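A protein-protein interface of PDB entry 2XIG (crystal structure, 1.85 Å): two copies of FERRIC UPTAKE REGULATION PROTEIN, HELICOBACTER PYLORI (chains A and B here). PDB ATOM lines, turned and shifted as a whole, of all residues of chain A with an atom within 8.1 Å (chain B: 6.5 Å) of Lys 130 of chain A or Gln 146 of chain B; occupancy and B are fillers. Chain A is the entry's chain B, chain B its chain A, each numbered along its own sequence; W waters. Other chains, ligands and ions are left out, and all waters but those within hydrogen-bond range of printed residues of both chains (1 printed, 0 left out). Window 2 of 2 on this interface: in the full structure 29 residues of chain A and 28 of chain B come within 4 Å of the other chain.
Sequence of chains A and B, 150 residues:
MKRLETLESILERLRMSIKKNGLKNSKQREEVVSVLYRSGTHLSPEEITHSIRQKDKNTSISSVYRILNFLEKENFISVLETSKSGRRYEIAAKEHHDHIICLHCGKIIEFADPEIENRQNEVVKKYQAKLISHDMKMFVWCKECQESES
N of Phe 139 of chain B lies within hydrogen-bond range of O of Ser 133 of chain A (2.8 Å).
N of Ile 132 of chain A lies within hydrogen-bond range of O of Phe 139 of chain B, 2.9 Å away.
The backbone carbonyl oxygen (O) of Trp 141 of chain B is in hydrogen-bond range of the backbone NH (N) of Lys 130 of chain A (2.9 Å).
NZ of Lys 143 of chain B is in hydrogen-bond range of OE1 of Gln 128 of chain A.
The side-chain amide oxygen (OE1) of Gln 146 of chain B lies close to the backbone carbonyl oxygen (O) of Trp 141 of chain B (3.3 Å).
The backbone carbonyl oxygen of Val 124 of chain A is in hydrogen-bond range of the backbone NH of Ala 129 of chain A (3.3 Å).
Val 124 of chain A touches Val 140 of chain B (CG1 to CG1, 3.6 Å).
Lys 143 of chain B touches Tyr 127 of chain A (CB to O, 3.6 Å).
Gln 128 of chain A touches Gln 146 of chain B.
Ala 129 of chain A touches Trp 141 of chain B (CA to O, 3.4 Å).
OE1 of Gln 146 of chain B touches C of Ala 129 of chain A (3.99 Å).
Lys 130 of chain A touches Val 140 of chain B (O to CA, 3.0 Å).
Gln 146 of chain B touches Lys 130 of chain A.
Leu 131 of chain A touches Phe 139 of chain B (CD1 to O, 3.7 Å).
Trp 141 of chain B touches Ile 132 of chain A.
Printed residues of chain B within 4 Å of Lys 130 of chain A: Val 140, Trp 141 and Gln 146.
Printed residues of chain A within 4 Å of Gln 146 of chain B: Gln 128, Ala 129 and Lys 130.
Of the printed residues of chain B, Val 124 of chain A touches Val 140 (3.6 Å).
Of the printed residues of chain A, Trp 141 of chain B touches Ala 129 (3.4 Å), Lys 130 (2.9 Å) and Ile 132 (3.5 Å).
Printed residues of chain A within 4 Å of Val 140 of chain B: Val 124 and Lys 130.
Of the printed residues of chain B, Ser 133 of chain A touches Phe 139.
Asn 121 of chain A touches none of the printed residues of chain B.
The nearest residue of chain B that does not touch Lys 130 of chain A is Phe 139 of chain B (4.2 Å).
The nearest printed residue of chain A that does not touch Gln 146 of chain B is Leu 131 of chain A (6.7 Å).
Printed residues of chain B that touch a printed residue of chain A: Phe 139, Val 140, Trp 141, Lys 143 and Gln 146.
Hydrophobic or aromatic side chains of chain B within 4 Å of the printed part of chain A: Phe 139, Val 140 and Trp 141.
Of the 11 printed residues of chain A, 8 touch a printed residue of chain B.
Hydrophobic or aromatic side chains of chain A that line the printed part of chain B: Val 124, Ala 129, Leu 131 and Ile 132.
Among the printed residues, no Asp or Glu carboxylate lies within 4 Å of a Lys or Arg side-chain nitrogen of the other chain.
No position is printed for both chains.
Of the 13 pairs that touch across the chains among the printed residues, none has its exchanged pair printed and touching as well.
Water W1 bridges O of Tyr 127 of chain A and N of Lys 143 of chain B.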
ATOM      1  N   GLN A 120      24.181 -33.033 -20.066  1.00  0.00           N
ATOM      2  CA  GLN A 120      22.929 -32.654 -19.425  1.00  0.00           C
ATOM      3  C   GLN A 120      21.909 -32.203 -20.463  1.00  0.00           C
ATOM      4  O   GLN A 120      20.726 -32.526 -20.370  1.00  0.00           O
ATOM      5  CB  GLN A 120      23.162 -31.538 -18.402  1.00  0.00           C
ATOM      6  CG  GLN A 120      23.809 -32.026 -17.106  1.00  0.00           C
ATOM      7  CD  GLN A 120      24.185 -30.884 -16.163  1.00  0.00           C
ATOM      8  OE1 GLN A 120      24.345 -29.741 -16.588  1.00  0.00           O
ATOM      9  NE2 GLN A 120      24.334 -31.198 -14.882  1.00  0.00           N
ATOM     10  N   ASN A 121      22.382 -31.439 -21.441  1.00  0.00           N
ATOM     11  CA  ASN A 121      21.530 -30.931 -22.510  1.00  0.00           C
ATOM     12  C   ASN A 121      21.040 -32.099 -23.354  1.00  0.00           C
ATOM     13  O   ASN A 121      19.861 -32.183 -23.694  1.00  0.00           O
ATOM     14  CB  ASN A 121      22.318 -29.941 -23.371  1.00  0.00           C
ATOM     15  CG  ASN A 121      21.483 -28.754 -23.821  1.00  0.00           C
ATOM     16  OD1 ASN A 121      20.261 -28.736 -23.666  1.00  0.00           O
ATOM     17  ND2 ASN A 121      22.147 -27.750 -24.379  1.00  0.00           N
ATOM     18  N   VAL A 124      18.223 -34.030 -21.609  1.00  0.00           N
ATOM     19  CA  VAL A 124      16.981 -33.266 -21.654  1.00  0.00           C
ATOM     20  C   VAL A 124      16.360 -33.295 -23.053  1.00  0.00           C
ATOM     21  O   VAL A 124      15.155 -33.493 -23.206  1.00  0.00           O
ATOM     22  CB  VAL A 124      17.204 -31.814 -21.197  1.00  0.00           C
ATOM     23  CG1 VAL A 124      15.936 -31.013 -21.338  1.00  0.00           C
ATOM     24  CG2 VAL A 124      17.673 -31.790 -19.759  1.00  0.00           C
ATOM     25  N   LYS A 125      17.193 -33.112 -24.072  1.00  0.00           N
ATOM     26  CA  LYS A 125      16.723 -33.152 -25.453  1.00  0.00           C
ATOM     27  C   LYS A 125      16.136 -34.511 -25.846  1.00  0.00           C
ATOM     28  O   LYS A 125      15.317 -34.595 -26.762  1.00  0.00           O
ATOM     29  CB  LYS A 125      17.837 -32.755 -26.419  1.00  0.00           C
ATOM     30  CG  LYS A 125      18.313 -31.325 -26.252  1.00  0.00           C
ATOM     31  CD  LYS A 125      19.142 -30.916 -27.449  1.00  0.00           C
ATOM     32  CE  LYS A 125      20.067 -29.767 -27.126  1.00  0.00           C
ATOM     33  NZ  LYS A 125      20.961 -29.500 -28.283  1.00  0.00           N
ATOM     34  N   TYR A 127      14.018 -35.851 -24.309  1.00  0.00           N
ATOM     35  CA  TYR A 127      12.612 -35.678 -23.952  1.00  0.00           C
ATOM     36  C   TYR A 127      12.002 -34.507 -24.710  1.00  0.00           C
ATOM     37  O   TYR A 127      10.865 -34.109 -24.456  1.00  0.00           O
ATOM     38  CB  TYR A 127      12.470 -35.473 -22.439  1.00  0.00           C
ATOM     39  CG  TYR A 127      12.994 -36.646 -21.645  1.00  0.00           C
ATOM     40  CD1 TYR A 127      12.214 -37.779 -21.450  1.00  0.00           C
ATOM     41  CD2 TYR A 127      14.279 -36.637 -21.117  1.00  0.00           C
ATOM     42  CE1 TYR A 127      12.691 -38.862 -20.742  1.00  0.00           C
ATOM     43  CE2 TYR A 127      14.766 -37.722 -20.407  1.00  0.00           C
ATOM     44  CZ  TYR A 127      13.964 -38.829 -20.223  1.00  0.00           C
ATOM     45  OH  TYR A 127      14.435 -39.912 -19.517  1.00  0.00           O
ATOM     46  N   GLN A 128      12.766 -33.965 -25.651  1.00  0.00           N
ATOM     47  CA  GLN A 128      12.338 -32.794 -26.397  1.00  0.00           C
ATOM     48  C   GLN A 128      11.988 -31.679 -25.417  1.00  0.00           C
ATOM     49  O   GLN A 128      11.019 -30.948 -25.606  1.00  0.00           O
ATOM     50  CB  GLN A 128      11.147 -33.143 -27.286  1.00  0.00           C
ATOM     51  CG  GLN A 128      11.350 -34.438 -28.070  1.00  0.00           C
ATOM     52  CD  GLN A 128      10.158 -34.795 -28.934  1.00  0.00           C
ATOM     53  OE1 GLN A 128       9.611 -33.946 -29.639  1.00  0.00           O
ATOM     54  NE2 GLN A 128       9.751 -36.059 -28.889  1.00  0.00           N
ATOM     55  N   ALA A 129      12.780 -31.575 -24.355  1.00  0.00           N
ATOM     56  CA  ALA A 129      12.653 -30.476 -23.412  1.00  0.00           C
ATOM     57  C   ALA A 129      13.730 -29.430 -23.698  1.00  0.00           C
ATOM     58  O   ALA A 129      14.645 -29.665 -24.487  1.00  0.00           O
ATOM     59  CB  ALA A 129      12.752 -30.987 -21.980  1.00  0.00           C
ATOM     60  N   LYS A 130      13.605 -28.265 -23.073  1.00  0.00           N
ATOM     61  CA  LYS A 130      14.581 -27.199 -23.237  1.00  0.00           C
ATOM     62  C   LYS A 130      15.232 -26.941 -21.887  1.00  0.00           C
ATOM     63  O   LYS A 130      14.543 -26.637 -20.912  1.00  0.00           O
ATOM     64  CB  LYS A 130      13.904 -25.924 -23.757  1.00  0.00           C
ATOM     65  CG  LYS A 130      14.833 -24.716 -23.901  1.00  0.00           C
ATOM     66  CD  LYS A 130      14.037 -23.447 -24.202  1.00  0.00           C
ATOM     67  CE  LYS A 130      14.887 -22.186 -24.079  1.00  0.00           C
ATOM     68  NZ  LYS A 130      15.523 -21.768 -25.362  1.00  0.00           N
ATOM     69  N   LEU A 131      16.553 -27.080 -21.827  1.00  0.00           N
ATOM     70  CA  LEU A 131      17.269 -26.891 -20.569  1.00  0.00           C
ATOM     71  C   LEU A 131      17.386 -25.409 -20.210  1.00  0.00           C
ATOM     72  O   LEU A 131      18.000 -24.626 -20.934  1.00  0.00           O
ATOM     73  CB  LEU A 131      18.650 -27.557 -20.613  1.00  0.00           C
ATOM     74  CG  LEU A 131      19.464 -27.487 -19.317  1.00  0.00           C
ATOM     75  CD1 LEU A 131      18.717 -28.152 -18.168  1.00  0.00           C
ATOM     76  CD2 LEU A 131      20.843 -28.108 -19.506  1.00  0.00           C
ATOM     77  N   ILE A 132      16.791 -25.027 -19.085  1.00  0.00           N
ATOM     78  CA  ILE A 132      16.832 -23.649 -18.615  1.00  0.00           C
ATOM     79  C   ILE A 132      17.944 -23.411 -17.591  1.00  0.00           C
ATOM     80  O   ILE A 132      18.720 -22.465 -17.702  1.00  0.00           O
ATOM     81  CB  ILE A 132      15.477 -23.232 -17.996  1.00  0.00           C
ATOM     82  CG1 ILE A 132      14.348 -23.369 -19.024  1.00  0.00           C
ATOM     83  CG2 ILE A 132      15.538 -21.817 -17.467  1.00  0.00           C
ATOM     84  CD1 ILE A 132      14.519 -22.464 -20.250  1.00  0.00           C
ATOM     85  N   SER A 133      18.004 -24.258 -16.572  1.00  0.00           N
ATOM     86  CA  SER A 133      19.064 -24.152 -15.588  1.00  0.00           C
ATOM     87  C   SER A 133      19.185 -25.492 -14.886  1.00  0.00           C
ATOM     88  O   SER A 133      18.431 -26.420 -15.156  1.00  0.00           O
ATOM     89  CB  SER A 133      18.770 -23.049 -14.567  1.00  0.00           C
ATOM     90  OG  SER A 133      17.707 -23.416 -13.703  1.00  0.00           O
ATOM     91  N   PHE B 139      16.264 -28.061 -14.639  1.00  0.00           N
ATOM     92  CA  PHE B 139      15.000 -27.345 -14.754  1.00  0.00           C
ATOM     93  C   PHE B 139      14.791 -26.977 -16.213  1.00  0.00           C
ATOM     94  O   PHE B 139      15.697 -26.464 -16.860  1.00  0.00           O
ATOM     95  CB  PHE B 139      15.006 -26.106 -13.861  1.00  0.00           C
ATOM     96  CG  PHE B 139      15.160 -26.419 -12.394  1.00  0.00           C
ATOM     97  CD1 PHE B 139      14.054 -26.704 -11.615  1.00  0.00           C
ATOM     98  CD2 PHE B 139      16.417 -26.420 -11.796  1.00  0.00           C
ATOM     99  CE1 PHE B 139      14.197 -26.995 -10.257  1.00  0.00           C
ATOM    100  CE2 PHE B 139      16.568 -26.706 -10.443  1.00  0.00           C
ATOM    101  CZ  PHE B 139      15.459 -26.991  -9.671  1.00  0.00           C
ATOM    102  N   VAL B 140      13.603 -27.271 -16.730  1.00  0.00           N
ATOM    103  CA  VAL B 140      13.364 -27.220 -18.167  1.00  0.00           C
ATOM    104  C   VAL B 140      12.012 -26.627 -18.520  1.00  0.00           C
ATOM    105  O   VAL B 140      11.186 -26.374 -17.646  1.00  0.00           O
ATOM    106  CB  VAL B 140      13.385 -28.648 -18.781  1.00  0.00           C
ATOM    107  CG1 VAL B 140      14.674 -29.382 -18.422  1.00  0.00           C
ATOM    108  CG2 VAL B 140      12.172 -29.450 -18.326  1.00  0.00           C
ATOM    109  N   TRP B 141      11.804 -26.404 -19.812  1.00  0.00           N
ATOM    110  CA  TRP B 141      10.464 -26.283 -20.364  1.00  0.00           C
ATOM    111  C   TRP B 141      10.191 -27.601 -21.070  1.00  0.00           C
ATOM    112  O   TRP B 141      10.884 -27.951 -22.028  1.00  0.00           O
ATOM    113  CB  TRP B 141      10.367 -25.137 -21.372  1.00  0.00           C
ATOM    114  CG  TRP B 141      10.684 -23.786 -20.823  1.00  0.00           C
ATOM    115  CD1 TRP B 141      10.745 -23.424 -19.509  1.00  0.00           C
ATOM    116  CD2 TRP B 141      10.944 -22.599 -21.580  1.00  0.00           C
ATOM    117  NE1 TRP B 141      11.057 -22.089 -19.402  1.00  0.00           N
ATOM    118  CE2 TRP B 141      11.180 -21.560 -20.660  1.00  0.00           C
ATOM    119  CE3 TRP B 141      11.014 -22.319 -22.947  1.00  0.00           C
ATOM    120  CZ2 TRP B 141      11.475 -20.262 -21.062  1.00  0.00           C
ATOM    121  CZ3 TRP B 141      11.308 -21.036 -23.346  1.00  0.00           C
ATOM    122  CH2 TRP B 141      11.535 -20.019 -22.407  1.00  0.00           C
ATOM    123  N   CYS B 142       9.203 -28.344 -20.585  1.00  0.00           N
ATOM    124  CA  CYS B 142       8.927 -29.671 -21.125  1.00  0.00           C
ATOM    125  C   CYS B 142       8.250 -29.609 -22.491  1.00  0.00           C
ATOM    126  O   CYS B 142       7.729 -28.568 -22.902  1.00  0.00           O
ATOM    127  CB  CYS B 142       8.070 -30.482 -20.153  1.00  0.00           C
ATOM    128  SG  CYS B 142       6.300 -30.120 -20.264  1.00  0.00           S
ATOM    129  N   LYS B 143       8.275 -30.736 -23.190  1.00  0.00           N
ATOM    130  CA  LYS B 143       7.745 -30.828 -24.542  1.00  0.00           C
ATOM    131  C   LYS B 143       6.330 -30.263 -24.640  1.00  0.00           C
ATOM    132  O   LYS B 143       6.021 -29.525 -25.559  1.00  0.00           O
ATOM    133  CB  LYS B 143       7.767 -32.284 -25.008  1.00  0.00           C
ATOM    134  CG  LYS B 143       6.759 -32.630 -26.090  1.00  0.00           C
ATOM    135  CD  LYS B 143       7.358 -32.575 -27.483  1.00  0.00           C
ATOM    136  CE  LYS B 143       6.378 -33.145 -28.497  1.00  0.00           C
ATOM    137  NZ  LYS B 143       6.971 -33.301 -29.846  1.00  0.00           N
ATOM    138  N   GLU B 144       5.485 -30.608 -23.678  1.00  0.00           N
ATOM    139  CA  GLU B 144       4.069 -30.255 -23.737  1.00  0.00           C
ATOM    140  C   GLU B 144       3.815 -28.777 -23.460  1.00  0.00           C
ATOM    141  O   GLU B 144       2.869 -28.189 -23.986  1.00  0.00           O
ATOM    142  CB  GLU B 144       3.264 -31.127 -22.767  1.00  0.00           C
ATOM    143  CG  GLU B 144       3.126 -32.578 -23.215  1.00  0.00           C
ATOM    144  CD  GLU B 144       4.431 -33.358 -23.127  1.00  0.00           C
ATOM    145  OE1 GLU B 144       5.276 -33.020 -22.271  1.00  0.00           O
ATOM    146  OE2 GLU B 144       4.610 -34.316 -23.911  1.00  0.00           O
ATOM    147  N   CYS B 145       4.662 -28.179 -22.630  1.00  0.00           N
ATOM    148  CA  CYS B 145       4.495 -26.777 -22.289  1.00  0.00           C
ATOM    149  C   CYS B 145       4.948 -25.887 -23.440  1.00  0.00           C
ATOM    150  O   CYS B 145       4.447 -24.774 -23.623  1.00  0.00           O
ATOM    151  CB  CYS B 145       5.242 -26.448 -20.995  1.00  0.00           C
ATOM    152  SG  CYS B 145       4.340 -26.938 -19.515  1.00  0.00           S
ATOM    153  N   GLN B 146       5.891 -26.396 -24.226  1.00  0.00           N
ATOM    154  CA  GLN B 146       6.426 -25.649 -25.355  1.00  0.00           C
ATOM    155  C   GLN B 146       5.492 -25.685 -26.558  1.00  0.00           C
ATOM    156  O   GLN B 146       5.573 -24.828 -27.440  1.00  0.00           O
ATOM    157  CB  GLN B 146       7.797 -26.194 -25.746  1.00  0.00           C
ATOM    158  CG  GLN B 146       8.878 -25.868 -24.738  1.00  0.00           C
ATOM    159  CD  GLN B 146      10.268 -26.122 -25.272  1.00  0.00           C
ATOM    160  OE1 GLN B 146      10.763 -27.250 -25.237  1.00  0.00           O
ATOM    161  NE2 GLN B 146      10.914 -25.067 -25.764  1.00  0.00           N
ATOM    162  N   GLU B 147       4.610 -26.677 -26.594  1.00  0.00           N
ATOM    163  CA  GLU B 147       3.699 -26.829 -27.723  1.00  0.00           C
ATOM    164  C   GLU B 147       2.520 -25.856 -27.703  1.00  0.00           C
ATOM    165  O   GLU B 147       1.813 -25.722 -26.701  1.00  0.00           O
ATOM    166  CB  GLU B 147       3.206 -28.274 -27.846  1.00  0.00           C
ATOM    167  CG  GLU B 147       4.103 -29.143 -28.712  1.00  0.00           C
ATOM    168  CD  GLU B 147       3.469 -30.476 -29.062  1.00  0.00           C
ATOM    169  OE1 GLU B 147       3.322 -31.324 -28.157  1.00  0.00           O
ATOM    170  OE2 GLU B 147       3.126 -30.678 -30.245  1.00  0.00           O
ATOM    171  N   SER B 148       2.327 -25.185 -28.833  1.00  0.00           N
ATOM    172  CA  SER B 148       1.215 -24.263 -29.022  1.00  0.00           C
ATOM    173  C   SER B 148      -0.129 -24.981 -28.949  1.00  0.00           C
ATOM    174  O   SER B 148      -1.163 -24.361 -28.699  1.00  0.00           O
ATOM    175  CB  SER B 148       1.361 -23.559 -30.370  1.00  0.00           C
ATOM    176  OG  SER B 148       1.974 -24.419 -31.317  1.00  0.00           O
HETATM  177  O   HOH W   1       9.544 -33.100 -22.218  1.00  0.00           O
